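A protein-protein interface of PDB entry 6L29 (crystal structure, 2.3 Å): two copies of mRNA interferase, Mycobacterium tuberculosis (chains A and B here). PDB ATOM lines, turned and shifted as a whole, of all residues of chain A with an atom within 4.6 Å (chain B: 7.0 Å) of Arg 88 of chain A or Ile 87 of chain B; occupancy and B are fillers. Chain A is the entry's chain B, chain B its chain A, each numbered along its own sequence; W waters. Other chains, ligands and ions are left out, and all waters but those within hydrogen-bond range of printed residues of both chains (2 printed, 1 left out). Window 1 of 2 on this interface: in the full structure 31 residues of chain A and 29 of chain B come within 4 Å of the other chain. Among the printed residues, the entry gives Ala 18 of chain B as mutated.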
ATOM      1  N   LEU A  16     -34.359  -9.294 -16.015  1.00  0.00           N
ATOM      2  CA  LEU A  16     -33.480  -9.696 -14.920  1.00  0.00           C
ATOM      3  C   LEU A  16     -32.603 -10.881 -15.305  1.00  0.00           C
ATOM      4  O   LEU A  16     -32.426 -11.814 -14.516  1.00  0.00           O
ATOM      5  CB  LEU A  16     -34.306 -10.017 -13.677  1.00  0.00           C
ATOM      6  CG  LEU A  16     -35.236  -8.894 -13.217  1.00  0.00           C
ATOM      7  CD1 LEU A  16     -36.063  -9.327 -12.013  1.00  0.00           C
ATOM      8  CD2 LEU A  16     -34.443  -7.624 -12.915  1.00  0.00           C
ATOM      9  N   ILE A  50     -32.229   2.652 -11.859  1.00  0.00           N
ATOM     10  CA  ILE A  50     -33.447   2.838 -11.084  1.00  0.00           C
ATOM     11  C   ILE A  50     -33.616   1.610 -10.205  1.00  0.00           C
ATOM     12  O   ILE A  50     -33.128   0.523 -10.526  1.00  0.00           O
ATOM     13  CB  ILE A  50     -34.699   3.060 -11.968  1.00  0.00           C
ATOM     14  CG1 ILE A  50     -34.964   1.841 -12.842  1.00  0.00           C
ATOM     15  CG2 ILE A  50     -34.548   4.316 -12.825  1.00  0.00           C
ATOM     16  CD1 ILE A  50     -36.361   1.794 -13.390  1.00  0.00           C
ATOM     17  N   THR A  51     -34.297   1.791  -9.082  1.00  0.00           N
ATOM     18  CA  THR A  51     -34.493   0.716  -8.122  1.00  0.00           C
ATOM     19  C   THR A  51     -35.918   0.207  -8.227  1.00  0.00           C
ATOM     20  O   THR A  51     -36.865   0.995  -8.213  1.00  0.00           O
ATOM     21  CB  THR A  51     -34.199   1.190  -6.701  1.00  0.00           C
ATOM     22  OG1 THR A  51     -32.859   1.698  -6.644  1.00  0.00           O
ATOM     23  CG2 THR A  51     -34.354   0.043  -5.724  1.00  0.00           C
ATOM     24  N   VAL A  52     -36.067  -1.110  -8.352  1.00  0.00           N
ATOM     25  CA  VAL A  52     -37.371  -1.716  -8.558  1.00  0.00           C
ATOM     26  C   VAL A  52     -37.579  -2.847  -7.558  1.00  0.00           C
ATOM     27  O   VAL A  52     -36.631  -3.383  -6.976  1.00  0.00           O
ATOM     28  CB  VAL A  52     -37.546  -2.236 -10.004  1.00  0.00           C
ATOM     29  CG1 VAL A  52     -37.419  -1.094 -11.008  1.00  0.00           C
ATOM     30  CG2 VAL A  52     -36.536  -3.334 -10.305  1.00  0.00           C
ATOM     31  N   GLN A  86     -36.603  -8.799  -2.732  1.00  0.00           N
ATOM     32  CA  GLN A  86     -35.977  -8.919  -4.040  1.00  0.00           C
ATOM     33  C   GLN A  86     -35.572  -7.566  -4.613  1.00  0.00           C
ATOM     34  O   GLN A  86     -35.191  -7.495  -5.787  1.00  0.00           O
ATOM     35  CB  GLN A  86     -36.914  -9.634  -5.018  1.00  0.00           C
ATOM     36  CG  GLN A  86     -37.122 -11.110  -4.730  1.00  0.00           C
ATOM     37  CD  GLN A  86     -35.904 -11.954  -5.078  1.00  0.00           C
ATOM     38  OE1 GLN A  86     -35.012 -11.517  -5.811  1.00  0.00           O
ATOM     39  NE2 GLN A  86     -35.865 -13.175  -4.552  1.00  0.00           N
ATOM     40  N   ILE A  87     -35.648  -6.502  -3.805  1.00  0.00           N
ATOM     41  CA  ILE A  87     -35.351  -5.153  -4.272  1.00  0.00           C
ATOM     42  C   ILE A  87     -34.034  -5.145  -5.038  1.00  0.00           C
ATOM     43  O   ILE A  87     -33.086  -5.864  -4.701  1.00  0.00           O
ATOM     44  CB  ILE A  87     -35.328  -4.180  -3.078  1.00  0.00           C
ATOM     45  CG1 ILE A  87     -35.068  -2.748  -3.540  1.00  0.00           C
ATOM     46  CG2 ILE A  87     -34.296  -4.614  -2.032  1.00  0.00           C
ATOM     47  CD1 ILE A  87     -35.360  -1.718  -2.485  1.00  0.00           C
ATOM     48  N   ARG A  88     -33.982  -4.350  -6.101  1.00  0.00           N
ATOM     49  CA  ARG A  88     -32.830  -4.406  -6.988  1.00  0.00           C
ATOM     50  C   ARG A  88     -32.721  -3.124  -7.802  1.00  0.00           C
ATOM     51  O   ARG A  88     -33.696  -2.697  -8.434  1.00  0.00           O
ATOM     52  CB  ARG A  88     -32.929  -5.617  -7.917  1.00  0.00           C
ATOM     53  CG  ARG A  88     -31.916  -5.570  -9.018  1.00  0.00           C
ATOM     54  CD  ARG A  88     -31.628  -6.931  -9.603  1.00  0.00           C
ATOM     55  NE  ARG A  88     -30.462  -6.831 -10.468  1.00  0.00           N
ATOM     56  CZ  ARG A  88     -30.070  -7.770 -11.313  1.00  0.00           C
ATOM     57  NH1 ARG A  88     -30.751  -8.903 -11.412  1.00  0.00           N
ATOM     58  NH2 ARG A  88     -28.993  -7.571 -12.059  1.00  0.00           N
ATOM     59  N   SER A  89     -31.532  -2.522  -7.781  1.00  0.00           N
ATOM     60  CA  SER A  89     -31.204  -1.413  -8.669  1.00  0.00           C
ATOM     61  C   SER A  89     -30.758  -1.967 -10.015  1.00  0.00           C
ATOM     62  O   SER A  89     -29.820  -2.768 -10.082  1.00  0.00           O
ATOM     63  CB  SER A  89     -30.109  -0.545  -8.053  1.00  0.00           C
ATOM     64  OG  SER A  89     -30.559   0.037  -6.841  1.00  0.00           O
ATOM     65  N   ILE A  90     -31.428  -1.549 -11.085  1.00  0.00           N
ATOM     66  CA  ILE A  90     -31.176  -2.074 -12.419  1.00  0.00           C
ATOM     67  C   ILE A  90     -30.774  -0.934 -13.344  1.00  0.00           C
ATOM     68  O   ILE A  90     -31.225   0.206 -13.193  1.00  0.00           O
ATOM     69  CB  ILE A  90     -32.406  -2.817 -12.989  1.00  0.00           C
ATOM     70  CG1 ILE A  90     -33.626  -1.897 -13.005  1.00  0.00           C
ATOM     71  CG2 ILE A  90     -32.711  -4.072 -12.182  1.00  0.00           C
ATOM     72  CD1 ILE A  90     -34.848  -2.520 -13.640  1.00  0.00           C
ATOM     73  N   ARG A  94     -32.306  -2.393 -18.920  1.00  0.00           N
ATOM     74  CA  ARG A  94     -33.090  -3.578 -18.587  1.00  0.00           C
ATOM     75  C   ARG A  94     -34.594  -3.348 -18.683  1.00  0.00           C
ATOM     76  O   ARG A  94     -35.361  -4.308 -18.553  1.00  0.00           O
ATOM     77  CB  ARG A  94     -32.755  -4.067 -17.175  1.00  0.00           C
ATOM     78  CG  ARG A  94     -31.392  -4.737 -17.025  1.00  0.00           C
ATOM     79  CD  ARG A  94     -31.238  -5.312 -15.618  1.00  0.00           C
ATOM     80  NE  ARG A  94     -29.857  -5.660 -15.309  1.00  0.00           N
ATOM     81  CZ  ARG A  94     -29.336  -6.874 -15.450  1.00  0.00           C
ATOM     82  NH1 ARG A  94     -30.083  -7.878 -15.899  1.00  0.00           N
ATOM     83  NH2 ARG A  94     -28.064  -7.080 -15.139  1.00  0.00           N
ATOM     84  N   LEU A 118     -35.691  -3.696   5.316  1.00  0.00           N
ATOM     85  CA  LEU A 118     -34.413  -3.000   5.428  1.00  0.00           C
ATOM     86  C   LEU A 118     -34.149  -2.454   6.827  1.00  0.00           C
ATOM     87  O   LEU A 118     -33.151  -1.751   7.023  1.00  0.00           O
ATOM     88  CB  LEU A 118     -34.339  -1.868   4.401  1.00  0.00           C
ATOM     89  CG  LEU A 118     -34.505  -2.320   2.948  1.00  0.00           C
ATOM     90  CD1 LEU A 118     -34.691  -1.135   2.011  1.00  0.00           C
ATOM     91  CD2 LEU A 118     -33.317  -3.153   2.522  1.00  0.00           C
ATOM     92  N   LEU B  16     -20.671  -9.685  -7.865  1.00  0.00           N
ATOM     93  CA  LEU B  16     -21.796  -9.218  -8.657  1.00  0.00           C
ATOM     94  C   LEU B  16     -21.663  -9.588 -10.124  1.00  0.00           C
ATOM     95  O   LEU B  16     -22.637  -9.449 -10.874  1.00  0.00           O
ATOM     96  CB  LEU B  16     -21.949  -7.708  -8.506  1.00  0.00           C
ATOM     97  CG  LEU B  16     -22.179  -7.297  -7.053  1.00  0.00           C
ATOM     98  CD1 LEU B  16     -21.912  -5.819  -6.893  1.00  0.00           C
ATOM     99  CD2 LEU B  16     -23.594  -7.654  -6.614  1.00  0.00           C
ATOM    100  N   ALA B  18     -21.864 -10.422 -13.615  1.00  0.00           N
ATOM    101  CA  ALA B  18     -22.385  -9.997 -14.915  1.00  0.00           C
ATOM    102  C   ALA B  18     -23.466  -8.944 -14.723  1.00  0.00           C
ATOM    103  O   ALA B  18     -24.610  -9.257 -14.378  1.00  0.00           O
ATOM    104  CB  ALA B  18     -22.925 -11.193 -15.690  1.00  0.00           C
ATOM    105  N   ALA B  19     -23.111  -7.689 -14.973  1.00  0.00           N
ATOM    106  CA  ALA B  19     -24.036  -6.582 -14.817  1.00  0.00           C
ATOM    107  C   ALA B  19     -24.105  -5.784 -16.109  1.00  0.00           C
ATOM    108  O   ALA B  19     -23.255  -5.904 -16.996  1.00  0.00           O
ATOM    109  CB  ALA B  19     -23.634  -5.669 -13.655  1.00  0.00           C
ATOM    110  N   ARG B  20     -25.140  -4.962 -16.196  1.00  0.00           N
ATOM    111  CA  ARG B  20     -25.406  -4.152 -17.371  1.00  0.00           C
ATOM    112  C   ARG B  20     -25.350  -2.680 -16.996  1.00  0.00           C
ATOM    113  O   ARG B  20     -25.673  -2.300 -15.866  1.00  0.00           O
ATOM    114  CB  ARG B  20     -26.782  -4.491 -17.966  1.00  0.00           C
ATOM    115  CG  ARG B  20     -26.861  -5.891 -18.563  1.00  0.00           C
ATOM    116  CD  ARG B  20     -28.306  -6.383 -18.684  1.00  0.00           C
ATOM    117  NE  ARG B  20     -28.959  -5.820 -19.862  1.00  0.00           N
ATOM    118  CZ  ARG B  20     -30.135  -6.228 -20.329  1.00  0.00           C
ATOM    119  NH1 ARG B  20     -30.654  -5.651 -21.401  1.00  0.00           N
ATOM    120  NH2 ARG B  20     -30.796  -7.208 -19.724  1.00  0.00           N
ATOM    121  N   GLU B  23     -24.775  -0.469 -13.497  1.00  0.00           N
ATOM    122  CA  GLU B  23     -24.866  -1.312 -12.312  1.00  0.00           C
ATOM    123  C   GLU B  23     -23.475  -1.639 -11.777  1.00  0.00           C
ATOM    124  O   GLU B  23     -22.533  -1.856 -12.546  1.00  0.00           O
ATOM    125  CB  GLU B  23     -25.604  -2.611 -12.642  1.00  0.00           C
ATOM    126  CG  GLU B  23     -27.071  -2.437 -12.979  1.00  0.00           C
ATOM    127  CD  GLU B  23     -27.679  -3.669 -13.646  1.00  0.00           C
ATOM    128  OE1 GLU B  23     -26.996  -4.712 -13.748  1.00  0.00           O
ATOM    129  OE2 GLU B  23     -28.851  -3.594 -14.063  1.00  0.00           O
ATOM    130  N   VAL B  33     -27.751  -4.723   4.527  1.00  0.00           N
ATOM    131  CA  VAL B  33     -28.796  -3.826   5.009  1.00  0.00           C
ATOM    132  C   VAL B  33     -30.136  -4.511   5.242  1.00  0.00           C
ATOM    133  O   VAL B  33     -31.035  -3.885   5.827  1.00  0.00           O
ATOM    134  CB  VAL B  33     -28.996  -2.613   4.070  1.00  0.00           C
ATOM    135  CG1 VAL B  33     -27.737  -1.754   4.024  1.00  0.00           C
ATOM    136  CG2 VAL B  33     -29.433  -3.062   2.676  1.00  0.00           C
ATOM    137  N   THR B  51     -30.007  -8.453   1.283  1.00  0.00           N
ATOM    138  CA  THR B  51     -29.943  -7.180   0.584  1.00  0.00           C
ATOM    139  C   THR B  51     -28.714  -6.417   1.052  1.00  0.00           C
ATOM    140  O   THR B  51     -28.453  -6.321   2.257  1.00  0.00           O
ATOM    141  CB  THR B  51     -31.218  -6.362   0.790  1.00  0.00           C
ATOM    142  OG1 THR B  51     -32.340  -7.145   0.377  1.00  0.00           O
ATOM    143  CG2 THR B  51     -31.176  -5.094  -0.048  1.00  0.00           C
ATOM    144  N   VAL B  52     -27.948  -5.907   0.090  1.00  0.00           N
ATOM    145  CA  VAL B  52     -26.683  -5.247   0.362  1.00  0.00           C
ATOM    146  C   VAL B  52     -26.635  -3.954  -0.436  1.00  0.00           C
ATOM    147  O   VAL B  52     -27.334  -3.773  -1.436  1.00  0.00           O
ATOM    148  CB  VAL B  52     -25.463  -6.136   0.013  1.00  0.00           C
ATOM    149  CG1 VAL B  52     -25.569  -7.510   0.685  1.00  0.00           C
ATOM    150  CG2 VAL B  52     -25.320  -6.282  -1.502  1.00  0.00           C
ATOM    151  N   VAL B  53     -25.782  -3.044   0.030  1.00  0.00           N
ATOM    152  CA  VAL B  53     -25.491  -1.774  -0.599  1.00  0.00           C
ATOM    153  C   VAL B  53     -24.038  -1.833  -1.083  1.00  0.00           C
ATOM    154  O   VAL B  53     -23.117  -1.894  -0.255  1.00  0.00           O
ATOM    155  CB  VAL B  53     -25.717  -0.602   0.366  1.00  0.00           C
ATOM    156  CG1 VAL B  53     -25.122   0.688  -0.182  1.00  0.00           C
ATOM    157  CG2 VAL B  53     -27.203  -0.451   0.650  1.00  0.00           C
ATOM    158  N   PRO B  54     -23.799  -1.883  -2.391  1.00  0.00           N
ATOM    159  CA  PRO B  54     -22.422  -1.967  -2.892  1.00  0.00           C
ATOM    160  C   PRO B  54     -21.609  -0.734  -2.536  1.00  0.00           C
ATOM    161  O   PRO B  54     -22.137   0.336  -2.220  1.00  0.00           O
ATOM    162  CB  PRO B  54     -22.604  -2.091  -4.409  1.00  0.00           C
ATOM    163  CG  PRO B  54     -23.959  -2.684  -4.573  1.00  0.00           C
ATOM    164  CD  PRO B  54     -24.788  -2.098  -3.459  1.00  0.00           C
ATOM    165  N   GLN B  83     -23.098   3.135  -1.876  1.00  0.00           N
ATOM    166  CA  GLN B  83     -24.016   3.696  -2.865  1.00  0.00           C
ATOM    167  C   GLN B  83     -25.410   3.115  -2.647  1.00  0.00           C
ATOM    168  O   GLN B  83     -25.715   2.019  -3.126  1.00  0.00           O
ATOM    169  CB  GLN B  83     -23.520   3.388  -4.272  1.00  0.00           C
ATOM    170  CG  GLN B  83     -22.149   3.946  -4.588  1.00  0.00           C
ATOM    171  CD  GLN B  83     -21.656   3.482  -5.935  1.00  0.00           C
ATOM    172  OE1 GLN B  83     -21.004   2.443  -6.045  1.00  0.00           O
ATOM    173  NE2 GLN B  83     -21.979   4.237  -6.974  1.00  0.00           N
ATOM    174  N   ALA B  84     -26.270   3.856  -1.942  1.00  0.00           N
ATOM    175  CA  ALA B  84     -27.634   3.379  -1.741  1.00  0.00           C
ATOM    176  C   ALA B  84     -28.409   3.283  -3.050  1.00  0.00           C
ATOM    177  O   ALA B  84     -29.363   2.506  -3.136  1.00  0.00           O
ATOM    178  CB  ALA B  84     -28.383   4.279  -0.755  1.00  0.00           C
ATOM    179  N   GLU B  85     -28.015   4.043  -4.075  1.00  0.00           N
ATOM    180  CA  GLU B  85     -28.655   3.929  -5.380  1.00  0.00           C
ATOM    181  C   GLU B  85     -28.264   2.650  -6.116  1.00  0.00           C
ATOM    182  O   GLU B  85     -28.811   2.383  -7.191  1.00  0.00           O
ATOM    183  CB  GLU B  85     -28.321   5.156  -6.237  1.00  0.00           C
ATOM    184  CG  GLU B  85     -26.950   5.122  -6.923  1.00  0.00           C
ATOM    185  CD  GLU B  85     -25.768   5.418  -5.988  1.00  0.00           C
ATOM    186  OE1 GLU B  85     -24.618   5.437  -6.479  1.00  0.00           O
ATOM    187  OE2 GLU B  85     -25.971   5.628  -4.772  1.00  0.00           O
ATOM    188  N   GLN B  86     -27.349   1.855  -5.560  1.00  0.00           N
ATOM    189  CA  GLN B  86     -26.960   0.567  -6.123  1.00  0.00           C
ATOM    190  C   GLN B  86     -27.470  -0.612  -5.302  1.00  0.00           C
ATOM    191  O   GLN B  86     -27.063  -1.752  -5.556  1.00  0.00           O
ATOM    192  CB  GLN B  86     -25.439   0.491  -6.260  1.00  0.00           C
ATOM    193  CG  GLN B  86     -24.865   1.424  -7.321  1.00  0.00           C
ATOM    194  CD  GLN B  86     -25.083   0.905  -8.731  1.00  0.00           C
ATOM    195  OE1 GLN B  86     -25.343  -0.282  -8.933  1.00  0.00           O
ATOM    196  NE2 GLN B  86     -24.980   1.792  -9.713  1.00  0.00           N
ATOM    197  N   ILE B  87     -28.366  -0.360  -4.340  1.00  0.00           N
ATOM    198  CA  ILE B  87     -28.868  -1.405  -3.453  1.00  0.00           C
ATOM    199  C   ILE B  87     -29.364  -2.597  -4.261  1.00  0.00           C
ATOM    200  O   ILE B  87     -30.028  -2.446  -5.293  1.00  0.00           O
ATOM    201  CB  ILE B  87     -29.982  -0.841  -2.551  1.00  0.00           C
ATOM    202  CG1 ILE B  87     -30.520  -1.920  -1.613  1.00  0.00           C
ATOM    203  CG2 ILE B  87     -31.112  -0.249  -3.395  1.00  0.00           C
ATOM    204  CD1 ILE B  87     -31.520  -1.406  -0.602  1.00  0.00           C
ATOM    205  N   ARG B  88     -29.032  -3.795  -3.792  1.00  0.00           N
ATOM    206  CA  ARG B  88     -29.364  -4.991  -4.545  1.00  0.00           C
ATOM    207  C   ARG B  88     -29.537  -6.177  -3.606  1.00  0.00           C
ATOM    208  O   ARG B  88     -28.759  -6.360  -2.664  1.00  0.00           O
ATOM    209  CB  ARG B  88     -28.284  -5.301  -5.586  1.00  0.00           C
ATOM    210  CG  ARG B  88     -28.617  -6.517  -6.409  1.00  0.00           C
ATOM    211  CD  ARG B  88     -27.597  -6.791  -7.480  1.00  0.00           C
ATOM    212  NE  ARG B  88     -27.865  -8.082  -8.100  1.00  0.00           N
ATOM    213  CZ  ARG B  88     -27.101  -8.631  -9.034  1.00  0.00           C
ATOM    214  NH1 ARG B  88     -26.021  -7.994  -9.460  1.00  0.00           N
ATOM    215  NH2 ARG B  88     -27.417  -9.814  -9.540  1.00  0.00           N
ATOM    216  N   SER B  89     -30.572  -6.969  -3.869  1.00  0.00           N
ATOM    217  CA  SER B  89     -30.726  -8.268  -3.232  1.00  0.00           C
ATOM    218  C   SER B  89     -29.909  -9.298  -3.999  1.00  0.00           C
ATOM    219  O   SER B  89     -30.027  -9.412  -5.222  1.00  0.00           O
ATOM    220  CB  SER B  89     -32.196  -8.684  -3.199  1.00  0.00           C
ATOM    221  OG  SER B  89     -32.985  -7.687  -2.572  1.00  0.00           O
ATOM    222  N   ARG B  94     -23.330 -15.339  -3.651  1.00  0.00           N
ATOM    223  CA  ARG B  94     -22.444 -14.259  -4.072  1.00  0.00           C
ATOM    224  C   ARG B  94     -21.559 -13.752  -2.942  1.00  0.00           C
ATOM    225  O   ARG B  94     -20.619 -12.995  -3.206  1.00  0.00           O
ATOM    226  CB  ARG B  94     -23.247 -13.087  -4.642  1.00  0.00           C
ATOM    227  CG  ARG B  94     -24.030 -13.401  -5.905  1.00  0.00           C
ATOM    228  CD  ARG B  94     -24.716 -12.144  -6.438  1.00  0.00           C
ATOM    229  NE  ARG B  94     -25.553 -12.409  -7.605  1.00  0.00           N
ATOM    230  CZ  ARG B  94     -25.115 -12.384  -8.859  1.00  0.00           C
ATOM    231  NH1 ARG B  94     -23.845 -12.108  -9.113  1.00  0.00           N
ATOM    232  NH2 ARG B  94     -25.948 -12.638  -9.858  1.00  0.00           N
ATOM    233  N   LEU B 114     -30.744   5.390   2.590  1.00  0.00           N
ATOM    234  CA  LEU B 114     -31.734   4.476   2.029  1.00  0.00           C
ATOM    235  C   LEU B 114     -33.127   5.094   2.045  1.00  0.00           C
ATOM    236  O   LEU B 114     -33.878   4.964   1.073  1.00  0.00           O
ATOM    237  CB  LEU B 114     -31.720   3.152   2.798  1.00  0.00           C
ATOM    238  CG  LEU B 114     -30.455   2.300   2.617  1.00  0.00           C
ATOM    239  CD1 LEU B 114     -30.374   1.184   3.646  1.00  0.00           C
ATOM    240  CD2 LEU B 114     -30.394   1.723   1.209  1.00  0.00           C
ATOM    241  N   HIS B 117     -33.141   7.701  -0.762  1.00  0.00           N
ATOM    242  CA  HIS B 117     -33.144   7.125  -2.101  1.00  0.00           C
ATOM    243  C   HIS B 117     -34.477   6.463  -2.425  1.00  0.00           C
ATOM    244  O   HIS B 117     -34.981   6.589  -3.547  1.00  0.00           O
ATOM    245  CB  HIS B 117     -32.015   6.110  -2.261  1.00  0.00           C
ATOM    246  CG  HIS B 117     -32.063   5.386  -3.569  1.00  0.00           C
ATOM    247  ND1 HIS B 117     -31.813   6.013  -4.771  1.00  0.00           N
ATOM    248  CD2 HIS B 117     -32.396   4.110  -3.872  1.00  0.00           C
ATOM    249  CE1 HIS B 117     -31.959   5.145  -5.756  1.00  0.00           C
ATOM    250  NE2 HIS B 117     -32.316   3.984  -5.238  1.00  0.00           N
ATOM    251  N   LEU B 118     -35.055   5.743  -1.466  1.00  0.00           N
ATOM    252  CA  LEU B 118     -36.291   5.014  -1.706  1.00  0.00           C
ATOM    253  C   LEU B 118     -37.533   5.806  -1.316  1.00  0.00           C
ATOM    254  O   LEU B 118     -38.652   5.294  -1.473  1.00  0.00           O
ATOM    255  CB  LEU B 118     -36.260   3.677  -0.959  1.00  0.00           C
ATOM    256  CG  LEU B 118     -35.067   2.791  -1.335  1.00  0.00           C
ATOM    257  CD1 LEU B 118     -34.905   1.664  -0.335  1.00  0.00           C
ATOM    258  CD2 LEU B 118     -35.185   2.243  -2.765  1.00  0.00           C
HETATM  259  O   HOH W   1     -31.305   3.146  -8.517  1.00  0.00           O
HETATM  260  O   HOH W   2     -28.374  -5.090 -10.620  1.00  0.00           O
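NE2 of His 117 of chain B lies within hydrogen-bond range of OG1 of Thr 51 of chain A.
The side-chain carboxylate of Glu 23 of chain B lies within salt-bridge range of the guanidinium group of Arg 94 of chain A.
O of Ile 87 of chain B is in hydrogen-bond range of N of Ser 89 of chain A (2.9 Å).
O of Leu 118 of chain A lies close to O of Val 33 of chain B, 3.2 Å away.
The backbone carbonyl oxygen (O) of Ile 87 of chain A lies within hydrogen-bond range of the side-chain hydroxyl (OG) of Ser 89 of chain B, at 2.8 Å.
O of Glu 85 of chain B lies within hydrogen-bond range of OG of Ser 89 of chain A (2.9 Å).
OE1 of Glu 23 of chain B lies within salt-bridge range of NH2 of Arg 88 of chain A (3.9 Å).
CG2 of Thr 51 of chain A touches CD2 of Leu 118 of chain B, at 3.8 Å.
Gln 86 of chain A touches Ser 89 of chain B (C to OG, 3.3 Å).
Ile 87 of chain A touches Thr 51 of chain B.
Ile 87 of chain A touches Arg 88 of chain B (O to C, 3.7 Å).
Leu 118 of chain B touches Ile 87 of chain A (CD2 to CD1, 3.97 Å).
Arg 88 of chain A touches Ile 87 of chain B (C to O, 3.7 Å).
Ile 90 of chain A touches Glu 23 of chain B.
Arg 20 of chain B touches Arg 94 of chain A (CD to CZ, 3.4 Å).
CG2 of Thr 51 of chain B touches CD2 of Leu 118 of chain A, 3.9 Å away.
CD1 of Leu 118 of chain A touches CD1 of Leu 118 of chain B, 3.7 Å away.
Water W2 lies within hydrogen-bond range of NE of Arg 88 of chain A, O of Ser 89 of chain A and OE1 of Glu 23 of chain B.
Water W1 bridges OG1 of Thr 51 of chain A and O of Glu 85 of chain B.
Ile 87 of chain A touches Thr 51 of chain B, but with the chains exchanged Thr 51 of chain A does not touch Ile 87 of chain B (4.003 Å).
Ile 87 of chain A touches Arg 88 of chain B, and with the chains exchanged Arg 88 of chain A touches Ile 87 of chain B.
Ile 87 of chain A touches Leu 118 of chain B, but with the chains exchanged Leu 118 of chain A does not touch Ile 87 of chain B (4.01 Å).
Arg 88 of chain A touches its own counterpart, Arg 88 of chain B.
Of the 11 printed residues of chain A, 8 touch a printed residue of chain B.
Hydrophobic or aromatic side chains of chain A within 4 Å of the printed part of chain B: Ile 87, Ile 90 and Leu 118.
Of the 21 printed residues of chain B, 11 touch a printed residue of chain A.
Among the printed residues, Asp or Glu carboxylates within 4 Å of a Lys or Arg side-chain nitrogen of the other chain: Arg 88 of chain A with Glu 23 of chain B and Arg 94 of chain A with Glu 23 of chain B.
Of chain B, only Glu 23, Ile 87 and Arg 88 come within 4 Å of Arg 88 of chain A.
Of the printed residues of chain A, Ile 87 of chain B touches Arg 88 and Ser 89.
Of the printed residues of chain A, His 117 of chain B touches Thr 51 (2.7 Å).
Of the printed residues of chain A, Glu 23 of chain B touches Arg 88, Ile 90 and Arg 94.
Printed residues of chain A within 4 Å of Ser 89 of chain B: Gln 86 (3.3 Å) and Ile 87 (2.8 Å).
Of the printed residues of chain B, Gln 86 of chain A touches Ser 89 (3.3 Å).
Of the printed residues of chain B, Leu 118 of chain A touches Val 33, Thr 51 and Leu 118.
The nearest residue of chain B that does not touch Arg 88 of chain A is Ser 89 of chain B (4.6 Å).
The nearest printed residue of chain A that does not touch Ile 87 of chain B is Thr 51 of chain A (4.003 Å).
The nearest printed residue of chain A that does not touch Glu 85 of chain B is Thr 51 of chain A (4.1 Å).
The backbone NH (N) of Val 33 of chain B lies within hydrogen-bond range of the backbone carbonyl oxygen (O) of Thr 51 of chain B (2.9 Å).
The backbone carbonyl oxygen of Val 52 of chain B lies within hydrogen-bond range of the backbone NH of Arg 88 of chain B (2.9 Å).
The backbone carbonyl oxygen (O) of Ile 50 of chain A sits at hydrogen-bond distance from the backbone NH (N) of Ile 90 of chain A, 2.7 Å away.
N of Arg 20 of chain B is in hydrogen-bond range of OE1 of Glu 23 of chain B (3.1 Å).
O of Arg 88 of chain A lies within hydrogen-bond range of N of Val 52 of chain A (2.9 Å).
The side-chain hydroxyl (OG) of Ser 89 of chain A sits at hydrogen-bond distance from the side-chain hydroxyl (OG1) of Thr 51 of chain A (2.8 Å).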
